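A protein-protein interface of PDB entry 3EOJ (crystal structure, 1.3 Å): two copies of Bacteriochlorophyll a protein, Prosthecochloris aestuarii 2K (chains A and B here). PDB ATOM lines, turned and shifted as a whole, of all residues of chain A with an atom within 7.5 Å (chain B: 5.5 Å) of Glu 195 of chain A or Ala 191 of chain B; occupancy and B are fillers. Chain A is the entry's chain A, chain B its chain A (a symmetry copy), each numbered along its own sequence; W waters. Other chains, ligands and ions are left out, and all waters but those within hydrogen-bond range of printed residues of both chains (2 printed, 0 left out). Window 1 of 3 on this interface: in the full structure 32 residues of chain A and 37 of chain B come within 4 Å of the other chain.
O of Gly 187 of chain B sits at hydrogen-bond distance from OG of Ser 230 of chain A.
Water W1 lies within hydrogen-bond range of the backbone carbonyl oxygen (O) of Phe 190 of chain B (2.7 Å), the side-chain amide nitrogen (ND2) of Asn 194 of chain A (2.9 Å) and the backbone NH (N) of Asn 194 of chain B (3.0 Å). Water W2 lies within hydrogen-bond range of O of Gly 187 of chain B, N of Ala 191 of chain B and N of Gly 197 of chain A.
Asn 194 of chain A touches Phe 190 of chain B, but with the chains exchanged Phe 190 of chain A does not touch Asn 194 of chain B (8.8 Å). Asn 194 of chain A touches Ala 191 of chain B, but with the chains exchanged Ala 191 of chain A does not touch Asn 194 of chain B (8.2 Å). Asn 194 of chain B touches its own counterpart, Asn 194 of chain A. Glu 195 of chain A touches Ala 191 of chain B, but with the chains exchanged Ala 191 of chain A does not touch Glu 195 of chain B (8.7 Å).
Hydrophobic or aromatic side chains of chain A that line the printed part of chain B: Val 232. Of the 10 printed residues of chain B, 4 touch a printed residue of chain A. Hydrophobic or aromatic side chains of chain B that line the printed part of chain A: Phe 190 and Ala 191. Among the printed residues, 8 pairs touch across the chains. Among the printed residues, no Asp or Glu carboxylate lies within 4 Å of a Lys or Arg side-chain nitrogen of the other chain.
Of the printed residues of chain B, Asn 194 of chain A touches Phe 190, Ala 191 and Asn 194. Printed residues of chain B within 4 Å of Gly 197 of chain A: Phe 190 (3.96 Å). Printed residues of chain A within 4 Å of Phe 190 of chain B: Asn 194, Gly 197 and Ser 230. Of the printed residues of chain A, Asn 194 of chain B touches Asn 194. The nearest printed residue of chain B that does not touch Glu 195 of chain A is Glu 195 of chain B (5.1 Å). The nearest printed residue of chain A that does not touch Ala 191 of chain B is Gly 197 of chain A (4.5 Å). The nearest printed residue of chain A that does not touch Asn 194 of chain B is Glu 195 of chain A (7.8 Å).
Among the printed residues, merely in contact across the chains: Asn 194 of chain A with Phe 190 of chain B (3.4 Å), Asn 194 of chain A with Ala 191 of chain B (3.4 Å), Asn 194 of chain A with Asn 194 of chain B (3.8 Å), Glu 195 of chain A with Ala 191 of chain B (3.7 Å), Gly 197 of chain A with Phe 190 of chain B (3.96 Å), Ser 230 of chain A with Phe 190 of chain B (3.8 Å) and Val 232 of chain A with Gly 187 of chain B (3.7 Å).
The backbone NH (N) of Ser 230 of chain A lies within hydrogen-bond range of the backbone carbonyl oxygen (O) of Gly 197 of chain A (3.1 Å).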
ATOM      1  N   ALA A 189     -19.356  21.465 -19.368  1.00  0.00           N
ATOM      2  CA  ALA A 189     -19.666  20.136 -18.867  1.00  0.00           C
ATOM      3  C   ALA A 189     -18.539  19.568 -18.017  1.00  0.00           C
ATOM      4  O   ALA A 189     -18.765  18.899 -17.025  1.00  0.00           O
ATOM      5  CB  ALA A 189     -20.027  19.186 -19.981  1.00  0.00           C
ATOM      6  N   PHE A 190     -17.276  19.827 -18.418  1.00  0.00           N
ATOM      7  CA  PHE A 190     -16.164  19.198 -17.712  1.00  0.00           C
ATOM      8  C   PHE A 190     -16.152  19.630 -16.242  1.00  0.00           C
ATOM      9  O   PHE A 190     -16.070  18.771 -15.358  1.00  0.00           O
ATOM     10  CB  PHE A 190     -14.850  19.551 -18.399  1.00  0.00           C
ATOM     11  CG  PHE A 190     -13.682  18.756 -17.866  1.00  0.00           C
ATOM     12  CD1 PHE A 190     -13.304  17.565 -18.475  1.00  0.00           C
ATOM     13  CD2 PHE A 190     -12.951  19.211 -16.772  1.00  0.00           C
ATOM     14  CE1 PHE A 190     -12.232  16.853 -18.001  1.00  0.00           C
ATOM     15  CE2 PHE A 190     -11.875  18.468 -16.307  1.00  0.00           C
ATOM     16  CZ  PHE A 190     -11.497  17.287 -16.920  1.00  0.00           C
ATOM     17  N   ALA A 191     -16.241  20.920 -15.970  1.00  0.00           N
ATOM     18  CA  ALA A 191     -16.236  21.413 -14.570  1.00  0.00           C
ATOM     19  C   ALA A 191     -17.419  20.896 -13.773  1.00  0.00           C
ATOM     20  O   ALA A 191     -17.320  20.711 -12.549  1.00  0.00           O
ATOM     21  CB  ALA A 191     -16.241  22.929 -14.575  1.00  0.00           C
ATOM     22  N   ALA A 192     -18.542  20.681 -14.441  1.00  0.00           N
ATOM     23  CA  ALA A 192     -19.733  20.218 -13.732  1.00  0.00           C
ATOM     24  C   ALA A 192     -19.531  18.840 -13.120  1.00  0.00           C
ATOM     25  O   ALA A 192     -20.209  18.519 -12.120  1.00  0.00           O
ATOM     26  CB  ALA A 192     -20.918  20.226 -14.664  1.00  0.00           C
ATOM     27  N   ILE A 193     -18.668  18.015 -13.685  1.00  0.00           N
ATOM     28  CA  ILE A 193     -18.442  16.678 -13.145  1.00  0.00           C
ATOM     29  C   ILE A 193     -18.050  16.781 -11.673  1.00  0.00           C
ATOM     30  O   ILE A 193     -18.709  16.242 -10.761  1.00  0.00           O
ATOM     31  CB  ILE A 193     -17.380  15.924 -13.970  1.00  0.00           C
ATOM     32  CG1 ILE A 193     -17.746  15.785 -15.453  1.00  0.00           C
ATOM     33  CG2 ILE A 193     -17.087  14.568 -13.323  1.00  0.00           C
ATOM     34  CD1 ILE A 193     -16.565  15.405 -16.325  1.00  0.00           C
ATOM     35  N   ASN A 194     -16.949  17.456 -11.366  1.00  0.00           N
ATOM     36  CA  ASN A 194     -16.495  17.551  -9.990  1.00  0.00           C
ATOM     37  C   ASN A 194     -17.459  18.285  -9.092  1.00  0.00           C
ATOM     38  O   ASN A 194     -17.555  17.970  -7.919  1.00  0.00           O
ATOM     39  CB  ASN A 194     -15.084  18.197  -9.929  1.00  0.00           C
ATOM     40  CG  ASN A 194     -14.327  17.712  -8.693  1.00  0.00           C
ATOM     41  OD1 ASN A 194     -13.903  16.550  -8.589  1.00  0.00           O
ATOM     42  ND2 ASN A 194     -14.095  18.592  -7.778  1.00  0.00           N
ATOM     43  N   GLU A 195     -18.191  19.265  -9.661  1.00  0.00           N
ATOM     44  CA  GLU A 195     -19.130  20.050  -8.888  1.00  0.00           C
ATOM     45  C   GLU A 195     -20.141  19.186  -8.159  1.00  0.00           C
ATOM     46  O   GLU A 195     -20.565  19.491  -7.066  1.00  0.00           O
ATOM     47  CB  GLU A 195     -19.864  21.013  -9.831  1.00  0.00           C
ATOM     48  CG  GLU A 195     -20.746  22.057  -9.176  1.00  0.00           C
ATOM     49  CD  GLU A 195     -20.030  23.270  -8.674  1.00  0.00           C
ATOM     50  OE1 GLU A 195     -18.791  23.356  -8.736  1.00  0.00           O
ATOM     51  OE2 GLU A 195     -20.720  24.241  -8.220  1.00  0.00           O
ATOM     52  N   GLY A 196     -20.558  18.103  -8.827  1.00  0.00           N
ATOM     53  CA  GLY A 196     -21.498  17.178  -8.280  1.00  0.00           C
ATOM     54  C   GLY A 196     -20.892  16.014  -7.533  1.00  0.00           C
ATOM     55  O   GLY A 196     -21.631  15.081  -7.211  1.00  0.00           O
ATOM     56  N   GLY A 197     -19.601  16.059  -7.200  1.00  0.00           N
ATOM     57  CA  GLY A 197     -18.962  14.912  -6.559  1.00  0.00           C
ATOM     58  C   GLY A 197     -18.938  13.689  -7.446  1.00  0.00           C
ATOM     59  O   GLY A 197     -18.913  12.557  -6.941  1.00  0.00           O
ATOM     60  N   GLN A 198     -18.895  13.899  -8.759  1.00  0.00           N
ATOM     61  CA  GLN A 198     -18.883  12.836  -9.726  1.00  0.00           C
ATOM     62  C   GLN A 198     -17.451  12.670 -10.248  1.00  0.00           C
ATOM     63  O   GLN A 198     -16.636  13.601 -10.200  1.00  0.00           O
ATOM     64  CB  GLN A 198     -19.888  13.197 -10.837  1.00  0.00           C
ATOM     65  CG  GLN A 198     -20.277  12.088 -11.811  1.00  0.00           C
ATOM     66  CD  GLN A 198     -21.503  12.436 -12.622  1.00  0.00           C
ATOM     67  OE1 GLN A 198     -22.021  13.558 -12.567  1.00  0.00           O
ATOM     68  NE2 GLN A 198     -22.000  11.494 -13.404  1.00  0.00           N
ATOM     69  N   SER A 230     -20.083  10.461  -4.911  1.00  0.00           N
ATOM     70  CA  SER A 230     -20.066  10.513  -3.466  1.00  0.00           C
ATOM     71  C   SER A 230     -21.448  10.577  -2.854  1.00  0.00           C
ATOM     72  O   SER A 230     -21.573  10.697  -1.616  1.00  0.00           O
ATOM     73  CB  SER A 230     -19.233  11.718  -2.991  1.00  0.00           C
ATOM     74  OG  SER A 230     -19.919  12.919  -3.412  1.00  0.00           O
ATOM     75  N   VAL A 232     -24.229  12.608  -4.221  1.00  0.00           N
ATOM     76  CA  VAL A 232     -25.038  13.629  -4.872  1.00  0.00           C
ATOM     77  C   VAL A 232     -25.544  13.132  -6.218  1.00  0.00           C
ATOM     78  O   VAL A 232     -26.631  13.522  -6.672  1.00  0.00           O
ATOM     79  CB  VAL A 232     -24.211  14.928  -5.024  1.00  0.00           C
ATOM     80  CG1 VAL A 232     -25.089  16.047  -5.583  1.00  0.00           C
ATOM     81  CG2 VAL A 232     -23.613  15.350  -3.709  1.00  0.00           C
ATOM     82  N   ILE A 293     -28.534  16.411  -8.528  1.00  0.00           N
ATOM     83  CA  ILE A 293     -27.730  16.915  -9.672  1.00  0.00           C
ATOM     84  C   ILE A 293     -28.437  18.045 -10.368  1.00  0.00           C
ATOM     85  O   ILE A 293     -27.745  19.006 -10.718  1.00  0.00           O
ATOM     86  CB  ILE A 293     -27.345  15.751 -10.587  1.00  0.00           C
ATOM     87  CG1 ILE A 293     -26.279  14.860  -9.927  1.00  0.00           C
ATOM     88  CG2 ILE A 293     -26.896  16.241 -11.953  1.00  0.00           C
ATOM     89  CD1 ILE A 293     -24.929  15.489  -9.773  1.00  0.00           C
ATOM     90  N   VAL A 296     -27.607  21.171  -8.298  1.00  0.00           N
ATOM     91  CA  VAL A 296     -26.190  21.510  -8.232  1.00  0.00           C
ATOM     92  C   VAL A 296     -25.734  22.036  -9.595  1.00  0.00           C
ATOM     93  O   VAL A 296     -25.050  23.044  -9.683  1.00  0.00           O
ATOM     94  CB  VAL A 296     -25.349  20.319  -7.751  1.00  0.00           C
ATOM     95  CG1 VAL A 296     -23.865  20.617  -7.875  1.00  0.00           C
ATOM     96  CG2 VAL A 296     -25.773  19.920  -6.333  1.00  0.00           C
ATOM     97  N   HIS A 297     -26.136  21.320 -10.673  1.00  0.00           N
ATOM     98  CA  HIS A 297     -25.711  21.767 -12.005  1.00  0.00           C
ATOM     99  C   HIS A 297     -26.367  23.080 -12.424  1.00  0.00           C
ATOM    100  O   HIS A 297     -25.684  23.978 -12.908  1.00  0.00           O
ATOM    101  CB  HIS A 297     -25.990  20.679 -13.029  1.00  0.00           C
ATOM    102  CG  HIS A 297     -25.076  19.497 -12.959  1.00  0.00           C
ATOM    103  ND1 HIS A 297     -25.106  18.509 -13.926  1.00  0.00           N
ATOM    104  CD2 HIS A 297     -24.140  19.169 -12.051  1.00  0.00           C
ATOM    105  CE1 HIS A 297     -24.189  17.635 -13.585  1.00  0.00           C
ATOM    106  NE2 HIS A 297     -23.567  17.989 -12.463  1.00  0.00           N
ATOM    107  N   GLY A 299     -27.189  25.238 -10.367  1.00  0.00           N
ATOM    108  CA  GLY A 299     -26.538  26.207  -9.512  1.00  0.00           C
ATOM    109  C   GLY A 299     -25.343  26.864 -10.169  1.00  0.00           C
ATOM    110  O   GLY A 299     -24.982  27.969  -9.755  1.00  0.00           O
ATOM    111  N   MET A 300     -24.750  26.204 -11.147  1.00  0.00           N
ATOM    112  CA  MET A 300     -23.638  26.778 -11.854  1.00  0.00           C
ATOM    113  C   MET A 300     -24.070  27.923 -12.789  1.00  0.00           C
ATOM    114  O   MET A 300     -23.182  28.651 -13.245  1.00  0.00           O
ATOM    115  CB  MET A 300     -22.914  25.677 -12.637  1.00  0.00           C
ATOM    116  CG  MET A 300     -22.401  24.556 -11.757  1.00  0.00           C
ATOM    117  SD  MET A 300     -21.578  23.241 -12.665  1.00  0.00           S
ATOM    118  CE  MET A 300     -19.995  24.002 -13.039  1.00  0.00           C
ATOM    119  N   LYS A 303     -26.698  31.984 -10.357  1.00  0.00           N
ATOM    120  CA  LYS A 303     -26.206  33.041  -9.479  1.00  0.00           C
ATOM    121  C   LYS A 303     -25.752  34.315 -10.174  1.00  0.00           C
ATOM    122  O   LYS A 303     -25.078  35.140  -9.558  1.00  0.00           O
ATOM    123  CB  LYS A 303     -25.040  32.525  -8.604  1.00  0.00           C
ATOM    124  CG  LYS A 303     -25.365  31.280  -7.758  1.00  0.00           C
ATOM    125  CD  LYS A 303     -24.156  30.955  -6.855  1.00  0.00           C
ATOM    126  CE  LYS A 303     -24.216  29.681  -6.114  1.00  0.00           C
ATOM    127  NZ  LYS A 303     -24.137  28.533  -7.067  1.00  0.00           N
ATOM    128  N   GLY B 187     -21.154  12.986  -0.097  1.00  0.00           N
ATOM    129  CA  GLY B 187     -22.005  14.109  -0.405  1.00  0.00           C
ATOM    130  C   GLY B 187     -21.194  15.259  -0.938  1.00  0.00           C
ATOM    131  O   GLY B 187     -20.287  15.026  -1.750  1.00  0.00           O
ATOM    132  N   PRO B 188     -21.436  16.490  -0.507  1.00  0.00           N
ATOM    133  CA  PRO B 188     -20.727  17.654  -1.019  1.00  0.00           C
ATOM    134  C   PRO B 188     -19.297  17.753  -0.520  1.00  0.00           C
ATOM    135  O   PRO B 188     -18.570  18.661  -0.956  1.00  0.00           O
ATOM    136  CB  PRO B 188     -21.532  18.864  -0.561  1.00  0.00           C
ATOM    137  CG  PRO B 188     -22.298  18.389   0.526  1.00  0.00           C
ATOM    138  CD  PRO B 188     -22.485  16.884   0.457  1.00  0.00           C
ATOM    139  N   ALA B 189     -18.880  16.863   0.368  1.00  0.00           N
ATOM    140  CA  ALA B 189     -17.501  16.918   0.825  1.00  0.00           C
ATOM    141  C   ALA B 189     -16.512  16.741  -0.317  1.00  0.00           C
ATOM    142  O   ALA B 189     -15.467  17.366  -0.357  1.00  0.00           O
ATOM    143  CB  ALA B 189     -17.233  15.920   1.923  1.00  0.00           C
ATOM    144  N   PHE B 190     -16.837  15.851  -1.279  1.00  0.00           N
ATOM    145  CA  PHE B 190     -15.865  15.552  -2.327  1.00  0.00           C
ATOM    146  C   PHE B 190     -15.534  16.816  -3.126  1.00  0.00           C
ATOM    147  O   PHE B 190     -14.353  17.122  -3.317  1.00  0.00           O
ATOM    148  CB  PHE B 190     -16.405  14.454  -3.234  1.00  0.00           C
ATOM    149  CG  PHE B 190     -15.367  13.931  -4.198  1.00  0.00           C
ATOM    150  CD1 PHE B 190     -14.591  12.826  -3.869  1.00  0.00           C
ATOM    151  CD2 PHE B 190     -15.184  14.531  -5.442  1.00  0.00           C
ATOM    152  CE1 PHE B 190     -13.661  12.343  -4.753  1.00  0.00           C
ATOM    153  CE2 PHE B 190     -14.231  14.027  -6.316  1.00  0.00           C
ATOM    154  CZ  PHE B 190     -13.465  12.922  -5.986  1.00  0.00           C
ATOM    155  N   ALA B 191     -16.538  17.547  -3.581  1.00  0.00           N
ATOM    156  CA  ALA B 191     -16.295  18.785  -4.363  1.00  0.00           C
ATOM    157  C   ALA B 191     -15.548  19.836  -3.562  1.00  0.00           C
ATOM    158  O   ALA B 191     -14.791  20.638  -4.130  1.00  0.00           O
ATOM    159  CB  ALA B 191     -17.622  19.345  -4.835  1.00  0.00           C
ATOM    160  N   ALA B 192     -15.766  19.858  -2.255  1.00  0.00           N
ATOM    161  CA  ALA B 192     -15.110  20.866  -1.426  1.00  0.00           C
ATOM    162  C   ALA B 192     -13.596  20.709  -1.432  1.00  0.00           C
ATOM    163  O   ALA B 192     -12.885  21.714  -1.206  1.00  0.00           O
ATOM    164  CB  ALA B 192     -15.653  20.805  -0.022  1.00  0.00           C
ATOM    165  N   ILE B 193     -13.082  19.512  -1.643  1.00  0.00           N
ATOM    166  CA  ILE B 193     -11.638  19.303  -1.649  1.00  0.00           C
ATOM    167  C   ILE B 193     -10.991  20.242  -2.666  1.00  0.00           C
ATOM    168  O   ILE B 193     -10.130  21.088  -2.348  1.00  0.00           O
ATOM    169  CB  ILE B 193     -11.297  17.827  -1.935  1.00  0.00           C
ATOM    170  CG1 ILE B 193     -11.915  16.852  -0.925  1.00  0.00           C
ATOM    171  CG2 ILE B 193      -9.778  17.656  -2.040  1.00  0.00           C
ATOM    172  CD1 ILE B 193     -11.914  15.415  -1.407  1.00  0.00           C
ATOM    173  N   ASN B 194     -11.351  20.130  -3.938  1.00  0.00           N
ATOM    174  CA  ASN B 194     -10.738  20.959  -4.960  1.00  0.00           C
ATOM    175  C   ASN B 194     -11.020  22.431  -4.784  1.00  0.00           C
ATOM    176  O   ASN B 194     -10.188  23.252  -5.125  1.00  0.00           O
ATOM    177  CB  ASN B 194     -11.168  20.482  -6.375  1.00  0.00           C
ATOM    178  CG  ASN B 194     -10.093  20.828  -7.405  1.00  0.00           C
ATOM    179  OD1 ASN B 194      -8.997  20.247  -7.439  1.00  0.00           O
ATOM    180  ND2 ASN B 194     -10.405  21.719  -8.284  1.00  0.00           N
ATOM    181  N   GLU B 195     -12.205  22.757  -4.228  1.00  0.00           N
ATOM    182  CA  GLU B 195     -12.588  24.140  -4.031  1.00  0.00           C
ATOM    183  C   GLU B 195     -11.559  24.917  -3.236  1.00  0.00           C
ATOM    184  O   GLU B 195     -11.331  26.085  -3.462  1.00  0.00           O
ATOM    185  CB  GLU B 195     -13.937  24.180  -3.301  1.00  0.00           C
ATOM    186  CG  GLU B 195     -14.601  25.537  -3.184  1.00  0.00           C
ATOM    187  CD  GLU B 195     -15.366  25.978  -4.390  1.00  0.00           C
ATOM    188  OE1 GLU B 195     -15.379  25.294  -5.429  1.00  0.00           O
ATOM    189  OE2 GLU B 195     -16.048  27.053  -4.321  1.00  0.00           O
ATOM    190  N   MET B 300     -19.471  27.744  -0.263  1.00  0.00           N
ATOM    191  CA  MET B 300     -20.230  26.821  -1.062  1.00  0.00           C
ATOM    192  C   MET B 300     -21.711  26.771  -0.646  1.00  0.00           C
ATOM    193  O   MET B 300     -22.500  26.215  -1.418  1.00  0.00           O
ATOM    194  CB  MET B 300     -19.590  25.430  -0.973  1.00  0.00           C
ATOM    195  CG  MET B 300     -18.149  25.404  -1.440  1.00  0.00           C
ATOM    196  SD  MET B 300     -17.375  23.787  -1.310  1.00  0.00           S
ATOM    197  CE  MET B 300     -18.101  22.931  -2.711  1.00  0.00           C
HETATM  198  O   HOH W   1     -12.700  17.841  -5.310  1.00  0.00           O
HETATM  199  O   HOH W   2     -19.243  16.549  -3.877  1.00  0.00           O
